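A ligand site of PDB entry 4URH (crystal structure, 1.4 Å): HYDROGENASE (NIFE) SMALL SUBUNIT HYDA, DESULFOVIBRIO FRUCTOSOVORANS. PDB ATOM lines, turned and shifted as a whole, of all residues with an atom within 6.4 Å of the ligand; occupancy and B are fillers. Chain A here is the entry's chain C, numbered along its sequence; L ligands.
The backbone carbonyl oxygen (O) of Arg 190 sits close to a sulfur (S2) of the ligand (3.7 Å).
Phe 194 touches the ligand.
Tyr 215 touches the ligand (CB to S4, 3.8 Å).
CA of Gly 221 touches S1 of the ligand (3.9 Å).
Pro 222 touches the ligand.
CG1 of Val 240 touches S3 of the ligand, 3.8 Å away.
Of the 25 residues printed, 12 come within 4 Å of the ligand.
The backbone NH of Leu 214 lies close to a sulfur (S3) of the ligand.
The side-chain sulfur of Cys 213 is bound to an iron atom (FE1) of the ligand.
An iron atom (FE2) of the ligand is bound by the side-chain sulfur (SG) of Cys 219.
N of Leu 191 sits close to S2 of the ligand (3.5 Å).
A ring nitrogen (ND1) of His 185 binds an iron atom (FE3) of the ligand, at 2.1 Å.
FE4 of the ligand is bound by SG of Cys 188, at 2.3 Å.
SG of Cys 188 lies close to N of Arg 190, at 3.3 Å.
The guanidinium group (NH1) of Arg 190 sits at hydrogen-bond distance from the backbone carbonyl oxygen (O) of Phe 212.
The guanidinium group of Arg 190 lies within hydrogen-bond range of the backbone carbonyl oxygen of Val 240, 3.1 Å away.
The backbone NH (N) of Cys 246 sits close to the side-chain sulfur (SG) of Cys 219 (3.5 Å).
O of Cys 219 is in hydrogen-bond range of NE2 of Gln 264 (2.8 Å).
The side-chain sulfur (SG) of Cys 219 lies close to the backbone NH (N) of Gly 221 (3.5 Å).
The backbone NH (N) of His 185 lies close to the backbone carbonyl oxygen (O) of Gly 221 (3.3 Å).
N of Cys 219 is in hydrogen-bond range of O of Leu 214, at 3.1 Å.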
ATOM      1  N   VAL A 184      -2.032  25.744 -23.558  1.00  0.00           N
ATOM      2  CA  VAL A 184      -0.914  25.997 -24.444  1.00  0.00           C
ATOM      3  C   VAL A 184      -0.747  24.841 -25.456  1.00  0.00           C
ATOM      4  O   VAL A 184      -0.648  25.043 -26.661  1.00  0.00           O
ATOM      5  CB  VAL A 184       0.375  26.196 -23.603  1.00  0.00           C
ATOM      6  CG1 VAL A 184       1.623  26.097 -24.504  1.00  0.00           C
ATOM      7  CG2 VAL A 184       0.327  27.520 -22.871  1.00  0.00           C
ATOM      8  N   HIS A 185      -0.748  23.604 -24.925  1.00  0.00           N
ATOM      9  CA  HIS A 185      -0.439  22.403 -25.688  1.00  0.00           C
ATOM     10  C   HIS A 185      -1.430  22.200 -26.857  1.00  0.00           C
ATOM     11  O   HIS A 185      -1.041  21.746 -27.958  1.00  0.00           O
ATOM     12  CB  HIS A 185      -0.502  21.236 -24.700  1.00  0.00           C
ATOM     13  CG  HIS A 185      -0.403  19.881 -25.298  1.00  0.00           C
ATOM     14  ND1 HIS A 185       0.785  19.368 -25.796  1.00  0.00           N
ATOM     15  CD2 HIS A 185      -1.317  18.880 -25.389  1.00  0.00           C
ATOM     16  CE1 HIS A 185       0.586  18.113 -26.180  1.00  0.00           C
ATOM     17  NE2 HIS A 185      -0.683  17.791 -25.943  1.00  0.00           N
ATOM     18  N   ASP A 186      -2.709  22.512 -26.616  1.00  0.00           N
ATOM     19  CA  ASP A 186      -3.727  22.286 -27.655  1.00  0.00           C
ATOM     20  C   ASP A 186      -3.510  23.112 -28.918  1.00  0.00           C
ATOM     21  O   ASP A 186      -3.991  22.746 -29.983  1.00  0.00           O
ATOM     22  CB  ASP A 186      -5.159  22.431 -27.106  1.00  0.00           C
ATOM     23  CG  ASP A 186      -5.536  21.250 -26.195  1.00  0.00           C
ATOM     24  OD1 ASP A 186      -4.842  20.183 -26.204  1.00  0.00           O
ATOM     25  OD2 ASP A 186      -6.523  21.371 -25.463  1.00  0.00           O
ATOM     26  N   CYS A 188      -0.220  24.103 -29.805  1.00  0.00           N
ATOM     27  CA  CYS A 188       1.209  24.042 -30.116  1.00  0.00           C
ATOM     28  C   CYS A 188       1.467  23.393 -31.481  1.00  0.00           C
ATOM     29  O   CYS A 188       0.976  22.279 -31.757  1.00  0.00           O
ATOM     30  CB  CYS A 188       1.955  23.273 -29.014  1.00  0.00           C
ATOM     31  SG  CYS A 188       3.725  23.138 -29.312  1.00  0.00           S
ATOM     32  N   PRO A 189       2.255  24.056 -32.343  1.00  0.00           N
ATOM     33  CA  PRO A 189       2.594  23.391 -33.634  1.00  0.00           C
ATOM     34  C   PRO A 189       3.374  22.073 -33.507  1.00  0.00           C
ATOM     35  O   PRO A 189       3.523  21.371 -34.492  1.00  0.00           O
ATOM     36  CB  PRO A 189       3.483  24.429 -34.332  1.00  0.00           C
ATOM     37  CG  PRO A 189       3.039  25.741 -33.742  1.00  0.00           C
ATOM     38  CD  PRO A 189       2.783  25.433 -32.287  1.00  0.00           C
ATOM     39  N   ARG A 190       3.902  21.741 -32.325  1.00  0.00           N
ATOM     40  CA  ARG A 190       4.603  20.460 -32.162  1.00  0.00           C
ATOM     41  C   ARG A 190       3.709  19.337 -31.717  1.00  0.00           C
ATOM     42  O   ARG A 190       4.181  18.224 -31.508  1.00  0.00           O
ATOM     43  CB  ARG A 190       5.799  20.588 -31.156  1.00  0.00           C
ATOM     44  CG  ARG A 190       6.768  21.679 -31.591  1.00  0.00           C
ATOM     45  CD  ARG A 190       8.092  21.689 -30.822  1.00  0.00           C
ATOM     46  NE  ARG A 190       8.956  22.780 -31.326  1.00  0.00           N
ATOM     47  CZ  ARG A 190      10.287  22.834 -31.177  1.00  0.00           C
ATOM     48  NH1 ARG A 190      10.945  21.841 -30.577  1.00  0.00           N
ATOM     49  NH2 ARG A 190      10.979  23.866 -31.692  1.00  0.00           N
ATOM     50  N   LEU A 191       2.422  19.632 -31.565  1.00  0.00           N
ATOM     51  CA  LEU A 191       1.439  18.634 -31.149  1.00  0.00           C
ATOM     52  C   LEU A 191       1.427  17.343 -31.987  1.00  0.00           C
ATOM     53  O   LEU A 191       1.353  16.259 -31.401  1.00  0.00           O
ATOM     54  CB  LEU A 191       0.050  19.281 -31.142  1.00  0.00           C
ATOM     55  CG  LEU A 191      -1.092  18.423 -30.593  1.00  0.00           C
ATOM     56  CD1 LEU A 191      -0.808  17.998 -29.169  1.00  0.00           C
ATOM     57  CD2 LEU A 191      -2.374  19.242 -30.651  1.00  0.00           C
ATOM     58  N   PRO A 192       1.580  17.434 -33.327  1.00  0.00           N
ATOM     59  CA  PRO A 192       1.702  16.161 -34.055  1.00  0.00           C
ATOM     60  C   PRO A 192       2.887  15.293 -33.610  1.00  0.00           C
ATOM     61  O   PRO A 192       2.801  14.039 -33.612  1.00  0.00           O
ATOM     62  CB  PRO A 192       1.898  16.613 -35.497  1.00  0.00           C
ATOM     63  CG  PRO A 192       1.111  17.927 -35.583  1.00  0.00           C
ATOM     64  CD  PRO A 192       1.466  18.593 -34.249  1.00  0.00           C
ATOM     65  N   HIS A 193       3.986  15.932 -33.206  1.00  0.00           N
ATOM     66  CA  HIS A 193       5.143  15.165 -32.705  1.00  0.00           C
ATOM     67  C   HIS A 193       4.773  14.506 -31.380  1.00  0.00           C
ATOM     68  O   HIS A 193       5.069  13.333 -31.174  1.00  0.00           O
ATOM     69  CB  HIS A 193       6.372  16.035 -32.525  1.00  0.00           C
ATOM     70  CG  HIS A 193       6.992  16.479 -33.803  1.00  0.00           C
ATOM     71  ND1 HIS A 193       7.415  15.587 -34.768  1.00  0.00           N
ATOM     72  CD2 HIS A 193       7.279  17.718 -34.263  1.00  0.00           C
ATOM     73  CE1 HIS A 193       7.950  16.270 -35.782  1.00  0.00           C
ATOM     74  NE2 HIS A 193       7.858  17.553 -35.508  1.00  0.00           N
ATOM     75  N   PHE A 194       4.102  15.275 -30.504  1.00  0.00           N
ATOM     76  CA  PHE A 194       3.628  14.698 -29.227  1.00  0.00           C
ATOM     77  C   PHE A 194       2.703  13.492 -29.476  1.00  0.00           C
ATOM     78  O   PHE A 194       2.892  12.418 -28.899  1.00  0.00           O
ATOM     79  CB  PHE A 194       2.933  15.801 -28.413  1.00  0.00           C
ATOM     80  CG  PHE A 194       2.309  15.340 -27.118  1.00  0.00           C
ATOM     81  CD1 PHE A 194       1.008  14.869 -27.094  1.00  0.00           C
ATOM     82  CD2 PHE A 194       3.017  15.449 -25.912  1.00  0.00           C
ATOM     83  CE1 PHE A 194       0.416  14.461 -25.897  1.00  0.00           C
ATOM     84  CE2 PHE A 194       2.435  15.067 -24.704  1.00  0.00           C
ATOM     85  CZ  PHE A 194       1.124  14.569 -24.691  1.00  0.00           C
ATOM     86  N   PHE A 199       9.804  12.761 -29.355  1.00  0.00           N
ATOM     87  CA  PHE A 199      10.283  13.665 -28.281  1.00  0.00           C
ATOM     88  C   PHE A 199      11.777  13.849 -28.363  1.00  0.00           C
ATOM     89  O   PHE A 199      12.504  12.877 -28.598  1.00  0.00           O
ATOM     90  CB  PHE A 199       9.978  13.066 -26.885  1.00  0.00           C
ATOM     91  CG  PHE A 199       8.520  12.747 -26.653  1.00  0.00           C
ATOM     92  CD1 PHE A 199       7.557  13.778 -26.621  1.00  0.00           C
ATOM     93  CD2 PHE A 199       8.094  11.426 -26.470  1.00  0.00           C
ATOM     94  CE1 PHE A 199       6.203  13.499 -26.384  1.00  0.00           C
ATOM     95  CE2 PHE A 199       6.740  11.147 -26.233  1.00  0.00           C
ATOM     96  CZ  PHE A 199       5.785  12.172 -26.197  1.00  0.00           C
ATOM     97  N   PHE A 212      11.298  18.453 -32.656  1.00  0.00           N
ATOM     98  CA  PHE A 212      10.421  17.467 -32.009  1.00  0.00           C
ATOM     99  C   PHE A 212       9.836  18.060 -30.713  1.00  0.00           C
ATOM    100  O   PHE A 212      10.355  19.056 -30.185  1.00  0.00           O
ATOM    101  CB  PHE A 212      11.220  16.188 -31.666  1.00  0.00           C
ATOM    102  CG  PHE A 212      11.356  15.205 -32.816  1.00  0.00           C
ATOM    103  CD1 PHE A 212      11.203  15.603 -34.154  1.00  0.00           C
ATOM    104  CD2 PHE A 212      11.684  13.868 -32.550  1.00  0.00           C
ATOM    105  CE1 PHE A 212      11.356  14.669 -35.191  1.00  0.00           C
ATOM    106  CE2 PHE A 212      11.809  12.946 -33.564  1.00  0.00           C
ATOM    107  CZ  PHE A 212      11.668  13.348 -34.895  1.00  0.00           C
ATOM    108  N   CYS A 213       8.801  17.403 -30.189  1.00  0.00           N
ATOM    109  CA  CYS A 213       8.118  17.831 -28.960  1.00  0.00           C
ATOM    110  C   CYS A 213       9.058  17.839 -27.748  1.00  0.00           C
ATOM    111  O   CYS A 213       9.964  16.994 -27.628  1.00  0.00           O
ATOM    112  CB  CYS A 213       6.918  16.944 -28.725  1.00  0.00           C
ATOM    113  SG  CYS A 213       6.145  17.099 -27.100  1.00  0.00           S
ATOM    114  N   LEU A 214       8.826  18.799 -26.839  1.00  0.00           N
ATOM    115  CA  LEU A 214       9.708  19.067 -25.700  1.00  0.00           C
ATOM    116  C   LEU A 214       9.178  18.483 -24.384  1.00  0.00           C
ATOM    117  O   LEU A 214       9.668  18.814 -23.299  1.00  0.00           O
ATOM    118  CB  LEU A 214       9.938  20.586 -25.583  1.00  0.00           C
ATOM    119  CG  LEU A 214      10.525  21.235 -26.831  1.00  0.00           C
ATOM    120  CD1 LEU A 214      10.572  22.757 -26.672  1.00  0.00           C
ATOM    121  CD2 LEU A 214      11.916  20.705 -27.168  1.00  0.00           C
ATOM    122  N   TYR A 215       8.208  17.574 -24.484  1.00  0.00           N
ATOM    123  CA  TYR A 215       7.622  16.963 -23.273  1.00  0.00           C
ATOM    124  C   TYR A 215       8.630  16.218 -22.373  1.00  0.00           C
ATOM    125  O   TYR A 215       8.587  16.310 -21.151  1.00  0.00           O
ATOM    126  CB  TYR A 215       6.447  16.068 -23.684  1.00  0.00           C
ATOM    127  CG  TYR A 215       5.552  15.644 -22.535  1.00  0.00           C
ATOM    128  CD1 TYR A 215       4.826  16.593 -21.820  1.00  0.00           C
ATOM    129  CD2 TYR A 215       5.366  14.297 -22.231  1.00  0.00           C
ATOM    130  CE1 TYR A 215       3.992  16.226 -20.775  1.00  0.00           C
ATOM    131  CE2 TYR A 215       4.528  13.920 -21.191  1.00  0.00           C
ATOM    132  CZ  TYR A 215       3.853  14.889 -20.456  1.00  0.00           C
ATOM    133  OH  TYR A 215       3.012  14.512 -19.440  1.00  0.00           O
ATOM    134  N   CYS A 219       8.396  20.045 -20.752  1.00  0.00           N
ATOM    135  CA  CYS A 219       7.387  21.011 -21.174  1.00  0.00           C
ATOM    136  C   CYS A 219       6.064  20.865 -20.416  1.00  0.00           C
ATOM    137  O   CYS A 219       5.475  19.757 -20.350  1.00  0.00           O
ATOM    138  CB  CYS A 219       7.140  20.900 -22.691  1.00  0.00           C
ATOM    139  SG  CYS A 219       6.011  22.204 -23.318  1.00  0.00           S
ATOM    140  N   LYS A 220       5.587  21.983 -19.853  1.00  0.00           N
ATOM    141  CA  LYS A 220       4.346  21.974 -19.055  1.00  0.00           C
ATOM    142  C   LYS A 220       3.125  22.453 -19.875  1.00  0.00           C
ATOM    143  O   LYS A 220       2.017  22.662 -19.326  1.00  0.00           O
ATOM    144  CB  LYS A 220       4.489  22.772 -17.767  1.00  0.00           C
ATOM    145  CG  LYS A 220       5.672  22.308 -16.894  1.00  0.00           C
ATOM    146  CD  LYS A 220       5.543  20.807 -16.550  1.00  0.00           C
ATOM    147  CE  LYS A 220       6.606  20.272 -15.595  1.00  0.00           C
ATOM    148  NZ  LYS A 220       8.008  20.751 -15.830  1.00  0.00           N
ATOM    149  N   GLY A 221       3.319  22.574 -21.187  1.00  0.00           N
ATOM    150  CA  GLY A 221       2.194  22.985 -22.065  1.00  0.00           C
ATOM    151  C   GLY A 221       0.912  22.181 -21.843  1.00  0.00           C
ATOM    152  O   GLY A 221      -0.157  22.746 -21.813  1.00  0.00           O
ATOM    153  N   PRO A 222       1.011  20.850 -21.662  1.00  0.00           N
ATOM    154  CA  PRO A 222      -0.209  20.055 -21.463  1.00  0.00           C
ATOM    155  C   PRO A 222      -1.025  20.340 -20.187  1.00  0.00           C
ATOM    156  O   PRO A 222      -2.149  19.835 -20.078  1.00  0.00           O
ATOM    157  CB  PRO A 222       0.313  18.595 -21.424  1.00  0.00           C
ATOM    158  CG  PRO A 222       1.594  18.636 -22.251  1.00  0.00           C
ATOM    159  CD  PRO A 222       2.209  19.958 -21.792  1.00  0.00           C
ATOM    160  N   TRP A 238       7.476  32.584 -29.397  1.00  0.00           N
ATOM    161  CA  TRP A 238       7.101  32.112 -28.077  1.00  0.00           C
ATOM    162  C   TRP A 238       8.058  30.997 -27.637  1.00  0.00           C
ATOM    163  O   TRP A 238       8.851  30.508 -28.440  1.00  0.00           O
ATOM    164  CB  TRP A 238       5.641  31.670 -28.038  1.00  0.00           C
ATOM    165  CG  TRP A 238       5.315  30.366 -28.709  1.00  0.00           C
ATOM    166  CD1 TRP A 238       5.323  30.091 -30.062  1.00  0.00           C
ATOM    167  CD2 TRP A 238       4.847  29.174 -28.067  1.00  0.00           C
ATOM    168  NE1 TRP A 238       4.907  28.793 -30.294  1.00  0.00           N
ATOM    169  CE2 TRP A 238       4.603  28.208 -29.090  1.00  0.00           C
ATOM    170  CE3 TRP A 238       4.645  28.791 -26.728  1.00  0.00           C
ATOM    171  CZ2 TRP A 238       4.152  26.896 -28.802  1.00  0.00           C
ATOM    172  CZ3 TRP A 238       4.191  27.486 -26.452  1.00  0.00           C
ATOM    173  CH2 TRP A 238       3.921  26.564 -27.501  1.00  0.00           C
ATOM    174  N   VAL A 240       8.355  27.750 -27.012  1.00  0.00           N
ATOM    175  CA  VAL A 240       8.542  26.455 -27.688  1.00  0.00           C
ATOM    176  C   VAL A 240       9.066  26.669 -29.128  1.00  0.00           C
ATOM    177  O   VAL A 240       9.876  25.882 -29.623  1.00  0.00           O
ATOM    178  CB  VAL A 240       7.226  25.621 -27.664  1.00  0.00           C
ATOM    179  CG1 VAL A 240       7.274  24.449 -28.673  1.00  0.00           C
ATOM    180  CG2 VAL A 240       6.996  25.126 -26.227  1.00  0.00           C
ATOM    181  N   HIS A 244      12.363  25.858 -26.391  1.00  0.00           N
ATOM    182  CA  HIS A 244      12.411  25.712 -24.935  1.00  0.00           C
ATOM    183  C   HIS A 244      11.070  25.261 -24.361  1.00  0.00           C
ATOM    184  O   HIS A 244      10.012  25.776 -24.787  1.00  0.00           O
ATOM    185  CB  HIS A 244      12.876  27.015 -24.248  1.00  0.00           C
ATOM    186  CG  HIS A 244      13.350  26.815 -22.845  1.00  0.00           C
ATOM    187  ND1 HIS A 244      12.489  26.581 -21.795  1.00  0.00           N
ATOM    188  CD2 HIS A 244      14.613  26.726 -22.327  1.00  0.00           C
ATOM    189  CE1 HIS A 244      13.189  26.379 -20.688  1.00  0.00           C
ATOM    190  NE2 HIS A 244      14.481  26.453 -20.983  1.00  0.00           N
ATOM    191  N   PRO A 245      11.085  24.299 -23.411  1.00  0.00           N
ATOM    192  CA  PRO A 245       9.801  23.922 -22.791  1.00  0.00           C
ATOM    193  C   PRO A 245       9.054  25.092 -22.116  1.00  0.00           C
ATOM    194  O   PRO A 245       9.670  26.058 -21.601  1.00  0.00           O
ATOM    195  CB  PRO A 245      10.222  22.893 -21.712  1.00  0.00           C
ATOM    196  CG  PRO A 245      11.712  23.045 -21.526  1.00  0.00           C
ATOM    197  CD  PRO A 245      12.213  23.505 -22.875  1.00  0.00           C
ATOM    198  N   CYS A 246       7.726  24.966 -22.072  1.00  0.00           N
ATOM    199  CA  CYS A 246       6.876  25.843 -21.265  1.00  0.00           C
ATOM    200  C   CYS A 246       7.147  25.516 -19.767  1.00  0.00           C
ATOM    201  O   CYS A 246       7.266  24.315 -19.396  1.00  0.00           O
ATOM    202  CB  CYS A 246       5.434  25.548 -21.643  1.00  0.00           C
ATOM    203  SG  CYS A 246       4.178  26.399 -20.641  1.00  0.00           S
ATOM    204  N   GLN A 264       9.455  15.864 -16.043  1.00  0.00           N
ATOM    205  CA  GLN A 264       8.018  15.725 -15.713  1.00  0.00           C
ATOM    206  C   GLN A 264       7.817  15.151 -14.302  1.00  0.00           C
ATOM    207  O   GLN A 264       6.681  14.913 -13.894  1.00  0.00           O
ATOM    208  CB  GLN A 264       7.344  14.835 -16.702  1.00  0.00           C
ATOM    209  CG  GLN A 264       7.276  15.389 -18.132  1.00  0.00           C
ATOM    210  CD  GLN A 264       6.442  16.695 -18.291  1.00  0.00           C
ATOM    211  OE1 GLN A 264       5.538  17.020 -17.491  1.00  0.00           O
ATOM    212  NE2 GLN A 264       6.761  17.447 -19.333  1.00  0.00           N
HETATM  213 FE1  LIG L   1       5.108  19.136 -26.942  1.00  0.00          FE
HETATM  214 FE2  LIG L   1       5.047  21.250 -25.144  1.00  0.00          FE
HETATM  215 FE3  LIG L   1       2.761  20.068 -26.023  1.00  0.00          FE
HETATM  216 FE4  LIG L   1       4.185  21.607 -27.684  1.00  0.00          FE
HETATM  217  S1  LIG L   1       3.131  22.326 -25.741  1.00  0.00           S
HETATM  218  S2  LIG L   1       3.254  19.549 -28.192  1.00  0.00           S
HETATM  219  S3  LIG L   1       6.330  21.096 -27.077  1.00  0.00           S
HETATM  220  S4  LIG L   1       4.347  19.096 -24.767  1.00  0.00           S
